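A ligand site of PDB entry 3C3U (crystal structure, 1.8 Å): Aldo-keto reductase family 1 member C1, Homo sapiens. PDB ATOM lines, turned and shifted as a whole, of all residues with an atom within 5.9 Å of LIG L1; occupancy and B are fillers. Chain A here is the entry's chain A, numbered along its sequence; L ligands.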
ATOM      1  N   TYR A  24     -15.163 -30.693   7.040  1.00  0.00           N
ATOM      2  CA  TYR A  24     -13.778 -31.148   7.093  1.00  0.00           C
ATOM      3  C   TYR A  24     -13.544 -32.052   8.304  1.00  0.00           C
ATOM      4  O   TYR A  24     -13.973 -31.733   9.414  1.00  0.00           O
ATOM      5  CB  TYR A  24     -12.822 -29.955   7.130  1.00  0.00           C
ATOM      6  CG  TYR A  24     -11.368 -30.338   7.261  1.00  0.00           C
ATOM      7  CD1 TYR A  24     -10.611 -30.643   6.140  1.00  0.00           C
ATOM      8  CD2 TYR A  24     -10.749 -30.395   8.501  1.00  0.00           C
ATOM      9  CE1 TYR A  24      -9.274 -30.995   6.251  1.00  0.00           C
ATOM     10  CE2 TYR A  24      -9.423 -30.741   8.621  1.00  0.00           C
ATOM     11  CZ  TYR A  24      -8.695 -31.044   7.499  1.00  0.00           C
ATOM     12  OH  TYR A  24      -7.366 -31.399   7.617  1.00  0.00           O
ATOM     13  N   ALA A  52     -14.970 -28.297   0.238  1.00  0.00           N
ATOM     14  CA  ALA A  52     -13.840 -27.815  -0.570  1.00  0.00           C
ATOM     15  C   ALA A  52     -13.237 -29.028  -1.302  1.00  0.00           C
ATOM     16  O   ALA A  52     -13.376 -30.184  -0.861  1.00  0.00           O
ATOM     17  CB  ALA A  52     -12.777 -27.174   0.353  1.00  0.00           C
ATOM     18  N   LEU A  54     -10.097 -29.581  -1.494  1.00  0.00           N
ATOM     19  CA  LEU A  54      -9.078 -30.047  -0.527  1.00  0.00           C
ATOM     20  C   LEU A  54      -9.559 -31.193   0.417  1.00  0.00           C
ATOM     21  O   LEU A  54      -8.772 -32.045   0.797  1.00  0.00           O
ATOM     22  CB  LEU A  54      -8.573 -28.910   0.357  1.00  0.00           C
ATOM     23  CG  LEU A  54      -7.364 -29.230   1.288  1.00  0.00           C
ATOM     24  CD1 LEU A  54      -6.111 -29.649   0.476  1.00  0.00           C
ATOM     25  CD2 LEU A  54      -7.043 -28.044   2.183  1.00  0.00           C
ATOM     26  N   TYR A  55     -10.843 -31.160   0.813  1.00  0.00           N
ATOM     27  CA  TYR A  55     -11.369 -32.022   1.874  1.00  0.00           C
ATOM     28  C   TYR A  55     -11.540 -33.477   1.491  1.00  0.00           C
ATOM     29  O   TYR A  55     -11.769 -34.330   2.383  1.00  0.00           O
ATOM     30  CB  TYR A  55     -12.710 -31.480   2.418  1.00  0.00           C
ATOM     31  CG  TYR A  55     -12.640 -30.068   2.950  1.00  0.00           C
ATOM     32  CD1 TYR A  55     -11.408 -29.411   3.091  1.00  0.00           C
ATOM     33  CD2 TYR A  55     -13.802 -29.398   3.347  1.00  0.00           C
ATOM     34  CE1 TYR A  55     -11.340 -28.092   3.607  1.00  0.00           C
ATOM     35  CE2 TYR A  55     -13.763 -28.072   3.835  1.00  0.00           C
ATOM     36  CZ  TYR A  55     -12.538 -27.438   3.972  1.00  0.00           C
ATOM     37  OH  TYR A  55     -12.514 -26.133   4.434  1.00  0.00           O
ATOM     38  N   LYS A  84     -14.625 -24.758  -2.676  1.00  0.00           N
ATOM     39  CA  LYS A  84     -13.435 -23.922  -2.743  1.00  0.00           C
ATOM     40  C   LYS A  84     -12.442 -24.438  -3.757  1.00  0.00           C
ATOM     41  O   LYS A  84     -12.222 -25.648  -3.896  1.00  0.00           O
ATOM     42  CB  LYS A  84     -12.754 -23.845  -1.372  1.00  0.00           C
ATOM     43  CG  LYS A  84     -13.748 -23.525  -0.189  1.00  0.00           C
ATOM     44  CD  LYS A  84     -12.971 -23.270   1.107  1.00  0.00           C
ATOM     45  CE  LYS A  84     -13.911 -23.188   2.358  1.00  0.00           C
ATOM     46  NZ  LYS A  84     -14.352 -24.592   2.744  1.00  0.00           N
ATOM     47  N   TRP A  86      -8.884 -24.984  -4.869  1.00  0.00           N
ATOM     48  CA  TRP A  86      -7.568 -25.216  -4.229  1.00  0.00           C
ATOM     49  C   TRP A  86      -6.367 -24.532  -4.973  1.00  0.00           C
ATOM     50  O   TRP A  86      -6.468 -24.133  -6.143  1.00  0.00           O
ATOM     51  CB  TRP A  86      -7.327 -26.739  -3.953  1.00  0.00           C
ATOM     52  CG  TRP A  86      -6.055 -26.934  -3.157  1.00  0.00           C
ATOM     53  CD1 TRP A  86      -4.905 -27.583  -3.573  1.00  0.00           C
ATOM     54  CD2 TRP A  86      -5.750 -26.365  -1.864  1.00  0.00           C
ATOM     55  NE1 TRP A  86      -3.922 -27.462  -2.581  1.00  0.00           N
ATOM     56  CE2 TRP A  86      -4.423 -26.710  -1.544  1.00  0.00           C
ATOM     57  CE3 TRP A  86      -6.492 -25.570  -0.940  1.00  0.00           C
ATOM     58  CZ2 TRP A  86      -3.821 -26.314  -0.336  1.00  0.00           C
ATOM     59  CZ3 TRP A  86      -5.883 -25.190   0.250  1.00  0.00           C
ATOM     60  CH2 TRP A  86      -4.561 -25.564   0.537  1.00  0.00           C
ATOM     61  N   HIS A 117      -9.634 -20.674  -2.003  1.00  0.00           N
ATOM     62  CA  HIS A 117      -9.393 -21.267  -0.683  1.00  0.00           C
ATOM     63  C   HIS A 117      -8.253 -20.587   0.140  1.00  0.00           C
ATOM     64  O   HIS A 117      -8.364 -20.403   1.359  1.00  0.00           O
ATOM     65  CB  HIS A 117      -9.110 -22.771  -0.848  1.00  0.00           C
ATOM     66  CG  HIS A 117      -9.369 -23.581   0.387  1.00  0.00           C
ATOM     67  ND1 HIS A 117      -9.741 -24.907   0.342  1.00  0.00           N
ATOM     68  CD2 HIS A 117      -9.290 -23.262   1.704  1.00  0.00           C
ATOM     69  CE1 HIS A 117      -9.892 -25.370   1.581  1.00  0.00           C
ATOM     70  NE2 HIS A 117      -9.615 -24.380   2.427  1.00  0.00           N
ATOM     71  N   GLN A 190     -13.876 -15.954   4.219  1.00  0.00           N
ATOM     72  CA  GLN A 190     -13.912 -17.023   5.230  1.00  0.00           C
ATOM     73  C   GLN A 190     -12.543 -17.175   5.935  1.00  0.00           C
ATOM     74  O   GLN A 190     -11.531 -17.512   5.288  1.00  0.00           O
ATOM     75  CB  GLN A 190     -14.339 -18.346   4.604  1.00  0.00           C
ATOM     76  CG  GLN A 190     -14.653 -19.444   5.689  1.00  0.00           C
ATOM     77  CD  GLN A 190     -14.948 -20.795   5.083  1.00  0.00           C
ATOM     78  OE1 GLN A 190     -15.920 -20.937   4.310  1.00  0.00           O
ATOM     79  NE2 GLN A 190     -14.165 -21.781   5.441  1.00  0.00           N
ATOM     80  N   HIS A 222     -10.099 -28.226  14.817  1.00  0.00           N
ATOM     81  CA  HIS A 222      -9.995 -29.674  14.965  1.00  0.00           C
ATOM     82  C   HIS A 222      -8.748 -30.064  15.750  1.00  0.00           C
ATOM     83  O   HIS A 222      -8.669 -31.162  16.300  1.00  0.00           O
ATOM     84  CB  HIS A 222      -9.984 -30.348  13.591  1.00  0.00           C
ATOM     85  CG  HIS A 222      -9.177 -29.630  12.563  1.00  0.00           C
ATOM     86  ND1 HIS A 222      -7.797 -29.549  12.619  1.00  0.00           N
ATOM     87  CD2 HIS A 222      -9.542 -28.938  11.450  1.00  0.00           C
ATOM     88  CE1 HIS A 222      -7.352 -28.854  11.592  1.00  0.00           C
ATOM     89  NE2 HIS A 222      -8.393 -28.476  10.868  1.00  0.00           N
ATOM     90  N   GLU A 224      -5.858 -30.726  14.652  1.00  0.00           N
ATOM     91  CA  GLU A 224      -5.095 -31.762  13.961  1.00  0.00           C
ATOM     92  C   GLU A 224      -3.618 -31.385  13.861  1.00  0.00           C
ATOM     93  O   GLU A 224      -3.268 -30.293  13.414  1.00  0.00           O
ATOM     94  CB  GLU A 224      -5.662 -32.001  12.558  1.00  0.00           C
ATOM     95  CG  GLU A 224      -4.969 -33.108  11.789  1.00  0.00           C
ATOM     96  CD  GLU A 224      -5.543 -33.299  10.401  1.00  0.00           C
ATOM     97  OE1 GLU A 224      -6.186 -32.351   9.883  1.00  0.00           O
ATOM     98  OE2 GLU A 224      -5.348 -34.382   9.817  1.00  0.00           O
ATOM     99  N   TRP A 227      -0.888 -29.401  11.752  1.00  0.00           N
ATOM    100  CA  TRP A 227      -1.547 -28.128  11.416  1.00  0.00           C
ATOM    101  C   TRP A 227      -1.731 -27.157  12.592  1.00  0.00           C
ATOM    102  O   TRP A 227      -1.578 -25.936  12.427  1.00  0.00           O
ATOM    103  CB  TRP A 227      -2.927 -28.442  10.834  1.00  0.00           C
ATOM    104  CG  TRP A 227      -2.818 -29.292   9.619  1.00  0.00           C
ATOM    105  CD1 TRP A 227      -3.048 -30.641   9.517  1.00  0.00           C
ATOM    106  CD2 TRP A 227      -2.401 -28.848   8.334  1.00  0.00           C
ATOM    107  NE1 TRP A 227      -2.816 -31.050   8.215  1.00  0.00           N
ATOM    108  CE2 TRP A 227      -2.418 -29.971   7.472  1.00  0.00           C
ATOM    109  CE3 TRP A 227      -2.010 -27.595   7.808  1.00  0.00           C
ATOM    110  CZ2 TRP A 227      -2.071 -29.884   6.112  1.00  0.00           C
ATOM    111  CZ3 TRP A 227      -1.677 -27.514   6.460  1.00  0.00           C
ATOM    112  CH2 TRP A 227      -1.700 -28.654   5.631  1.00  0.00           C
ATOM    113  N   LEU A 306      -4.708 -22.128  13.190  1.00  0.00           N
ATOM    114  CA  LEU A 306      -4.341 -22.588  11.854  1.00  0.00           C
ATOM    115  C   LEU A 306      -3.439 -21.557  11.152  1.00  0.00           C
ATOM    116  O   LEU A 306      -3.906 -20.745  10.358  1.00  0.00           O
ATOM    117  CB  LEU A 306      -5.593 -22.918  11.014  1.00  0.00           C
ATOM    118  CG  LEU A 306      -5.319 -23.933   9.883  1.00  0.00           C
ATOM    119  CD1 LEU A 306      -5.081 -25.385  10.436  1.00  0.00           C
ATOM    120  CD2 LEU A 306      -6.443 -23.889   8.851  1.00  0.00           C
ATOM    121  N   LEU A 308      -1.203 -22.148   8.938  1.00  0.00           N
ATOM    122  CA  LEU A 308      -0.876 -22.614   7.571  1.00  0.00           C
ATOM    123  C   LEU A 308       0.546 -22.177   7.192  1.00  0.00           C
ATOM    124  O   LEU A 308       0.841 -21.850   6.014  1.00  0.00           O
ATOM    125  CB  LEU A 308      -1.930 -22.141   6.554  1.00  0.00           C
ATOM    126  CG  LEU A 308      -3.364 -22.628   6.895  1.00  0.00           C
ATOM    127  CD1 LEU A 308      -4.441 -21.997   5.976  1.00  0.00           C
ATOM    128  CD2 LEU A 308      -3.446 -24.160   6.896  1.00  0.00           C
ATOM    129  N   PHE A 311       2.995 -22.867   4.264  1.00  0.00           N
ATOM    130  CA  PHE A 311       2.887 -22.020   3.055  1.00  0.00           C
ATOM    131  C   PHE A 311       3.503 -20.619   3.211  1.00  0.00           C
ATOM    132  O   PHE A 311       3.271 -19.762   2.366  1.00  0.00           O
ATOM    133  CB  PHE A 311       1.417 -21.868   2.626  1.00  0.00           C
ATOM    134  CG  PHE A 311       0.699 -23.164   2.349  1.00  0.00           C
ATOM    135  CD1 PHE A 311       1.110 -23.982   1.291  1.00  0.00           C
ATOM    136  CD2 PHE A 311      -0.382 -23.554   3.131  1.00  0.00           C
ATOM    137  CE1 PHE A 311       0.445 -25.179   1.024  1.00  0.00           C
ATOM    138  CE2 PHE A 311      -1.052 -24.767   2.883  1.00  0.00           C
ATOM    139  CZ  PHE A 311      -0.643 -25.573   1.812  1.00  0.00           C
HETATM  140  O1  LIG L   1     -10.039 -25.626   4.898  1.00  0.00           O
HETATM  141  C1  LIG L   1      -9.662 -26.323   5.867  1.00  0.00           C
HETATM  142  O2  LIG L   1     -10.417 -26.904   6.661  1.00  0.00           O
HETATM  143  C2  LIG L   1      -8.204 -26.594   6.024  1.00  0.00           C
HETATM  144  C3  LIG L   1      -7.326 -26.121   5.078  1.00  0.00           C
HETATM  145  C4  LIG L   1      -7.762 -27.341   7.101  1.00  0.00           C
HETATM  146  O3  LIG L   1      -8.601 -27.825   8.053  1.00  0.00           O
HETATM  147  C5  LIG L   1      -6.413 -27.604   7.206  1.00  0.00           C
HETATM  148 CL1  LIG L   1      -5.876 -28.600   8.559  1.00  0.00          CL
HETATM  149  C6  LIG L   1      -5.491 -27.166   6.292  1.00  0.00           C
HETATM  150  C7  LIG L   1      -5.977 -26.403   5.238  1.00  0.00           C
HETATM  151 CL2  LIG L   1      -4.837 -25.821   4.023  1.00  0.00          CL
HETATM  152  P1  LG2 L   2     -14.587 -26.389  14.586  1.00  0.00           P
HETATM  153  O1  LG2 L   2     -13.856 -25.245  15.175  1.00  0.00           O
HETATM  154  O2  LG2 L   2     -15.925 -26.192  13.982  1.00  0.00           O
HETATM  155  O3  LG2 L   2     -14.800 -27.518  15.719  1.00  0.00           O
HETATM  156  C1  LG2 L   2     -13.713 -28.181  16.324  1.00  0.00           C
HETATM  157  C2  LG2 L   2     -14.146 -29.466  17.038  1.00  0.00           C
HETATM  158  O4  LG2 L   2     -15.166 -29.197  17.968  1.00  0.00           O
HETATM  159  C3  LG2 L   2     -14.703 -30.574  16.144  1.00  0.00           C
HETATM  160  O5  LG2 L   2     -13.662 -31.512  16.014  1.00  0.00           O
HETATM  161  C4  LG2 L   2     -15.835 -31.201  16.928  1.00  0.00           C
HETATM  162  O6  LG2 L   2     -15.600 -32.590  17.276  1.00  0.00           O
HETATM  163  C5  LG2 L   2     -15.958 -30.364  18.197  1.00  0.00           C
HETATM  164  N1  LG2 L   2     -17.351 -29.913  18.488  1.00  0.00           N
HETATM  165  C6  LG2 L   2     -18.337 -29.590  17.613  1.00  0.00           C
HETATM  166  N2  LG2 L   2     -19.445 -29.233  18.290  1.00  0.00           N
HETATM  167  C7  LG2 L   2     -19.158 -29.338  19.613  1.00  0.00           C
HETATM  168  C8  LG2 L   2     -19.878 -29.129  20.806  1.00  0.00           C
HETATM  169  N3  LG2 L   2     -21.159 -28.697  20.824  1.00  0.00           N
HETATM  170  N4  LG2 L   2     -19.242 -29.341  21.992  1.00  0.00           N
HETATM  171  C9  LG2 L   2     -17.989 -29.773  22.052  1.00  0.00           C
HETATM  172  N5  LG2 L   2     -17.250 -29.989  20.938  1.00  0.00           N
HETATM  173  C10 LG2 L   2     -17.833 -29.777  19.717  1.00  0.00           C
HETATM  174  O7  LG2 L   2     -13.723 -27.239  13.505  1.00  0.00           O
HETATM  175  P2  LG2 L   2     -12.911 -26.853  12.185  1.00  0.00           P
HETATM  176  O8  LG2 L   2     -11.519 -26.389  12.513  1.00  0.00           O
HETATM  177  O9  LG2 L   2     -13.078 -28.069  11.304  1.00  0.00           O
HETATM  178  O10 LG2 L   2     -13.689 -25.628  11.530  1.00  0.00           O
HETATM  179  C11 LG2 L   2     -15.019 -25.821  11.012  1.00  0.00           C
HETATM  180  C12 LG2 L   2     -15.055 -25.821   9.491  1.00  0.00           C
HETATM  181  O11 LG2 L   2     -14.629 -24.562   8.866  1.00  0.00           O
HETATM  182  C13 LG2 L   2     -14.269 -26.931   8.774  1.00  0.00           C
HETATM  183  O12 LG2 L   2     -14.860 -28.231   8.893  1.00  0.00           O
HETATM  184  C14 LG2 L   2     -14.293 -26.426   7.351  1.00  0.00           C
HETATM  185  O13 LG2 L   2     -15.616 -26.683   6.780  1.00  0.00           O
HETATM  186  C15 LG2 L   2     -14.062 -24.910   7.596  1.00  0.00           C
HETATM  187  N6  LG2 L   2     -12.623 -24.514   7.634  1.00  0.00           N
HETATM  188  C16 LG2 L   2     -12.125 -23.822   6.601  1.00  0.00           C
HETATM  189  C17 LG2 L   2     -10.788 -23.430   6.543  1.00  0.00           C
HETATM  190  C18 LG2 L   2     -10.267 -22.628   5.385  1.00  0.00           C
HETATM  191  O14 LG2 L   2      -9.055 -22.515   5.198  1.00  0.00           O
HETATM  192  N7  LG2 L   2     -11.207 -22.008   4.654  1.00  0.00           N
HETATM  193  C19 LG2 L   2      -9.924 -23.737   7.618  1.00  0.00           C
HETATM  194  C20 LG2 L   2     -10.452 -24.445   8.705  1.00  0.00           C
HETATM  195  C21 LG2 L   2     -11.803 -24.820   8.694  1.00  0.00           C
HETATM  196  P3  LG2 L   2     -16.772 -33.676  16.964  1.00  0.00           P
HETATM  197  O15 LG2 L   2     -16.799 -33.844  15.451  1.00  0.00           O
HETATM  198  O16 LG2 L   2     -16.189 -34.904  17.671  1.00  0.00           O
HETATM  199  O17 LG2 L   2     -18.106 -33.164  17.503  1.00  0.00           O
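O12 of LG2 L2 sits at hydrogen-bond distance from N of Tyr 24 (3.1 Å).
NE2 of His 222 sits at hydrogen-bond distance from O3 of LIG L1, at 2.9 Å.
N7 of LG2 L2 lies close to NE2 of Gln 190, 3.1 Å away.
The backbone NH of His 222 sits at hydrogen-bond distance from an oxygen (O8) of LG2 L2 (3.3 Å).
O1 of LIG L1 lies within hydrogen-bond range of NE2 of His 117.
A ring nitrogen (NE2) of His 117 lies within hydrogen-bond range of an oxygen (O14) of LG2 L2, 3.4 Å away.
OH of Tyr 55 lies within hydrogen-bond range of O1 of LIG L1.
The side-chain amino group of Lys 84 is in hydrogen-bond range of the side-chain hydroxyl of Tyr 55 (2.9 Å).
A ring nitrogen (ND1) of His 222 sits at hydrogen-bond distance from the backbone NH (N) of Glu 224.
The side-chain carboxylate (OE1) of Glu 224 lies within hydrogen-bond range of the side-chain hydroxyl (OH) of Tyr 24 (2.7 Å).
CE2 of Tyr 24 touches O3 of LIG L1 (3.1 Å).
CD2 of Leu 54 touches C3 of LIG L1 (3.5 Å).
CH2 of Trp 86 touches CL2 of LIG L1, at 3.5 Å.
OE1 of Glu 224 touches CL1 of LIG L1, at 3.99 Å.
Trp 227 touches LIG L1 (CG to CL1, 3.3 Å).
CD1 of Leu 306 touches CL1 of LIG L1, 3.8 Å away.
CD2 of Leu 308 touches CL2 of LIG L1, 3.6 Å away.
Hydrophobic or aromatic side chains within 4 Å of LIG L1: Tyr 24, Leu 54, Tyr 55, Trp 86, His 117, His 222, Trp 227, Leu 306 and Leu 308.
Ten residues have an atom within 4 Å of LIG L1: Tyr 24, Leu 54, Tyr 55, Trp 86, His 117, His 222, Glu 224, Trp 227, Leu 306 and Leu 308.
The nearest printed residue that does not touch LIG L1 is Phe 311 (4.1 Å).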
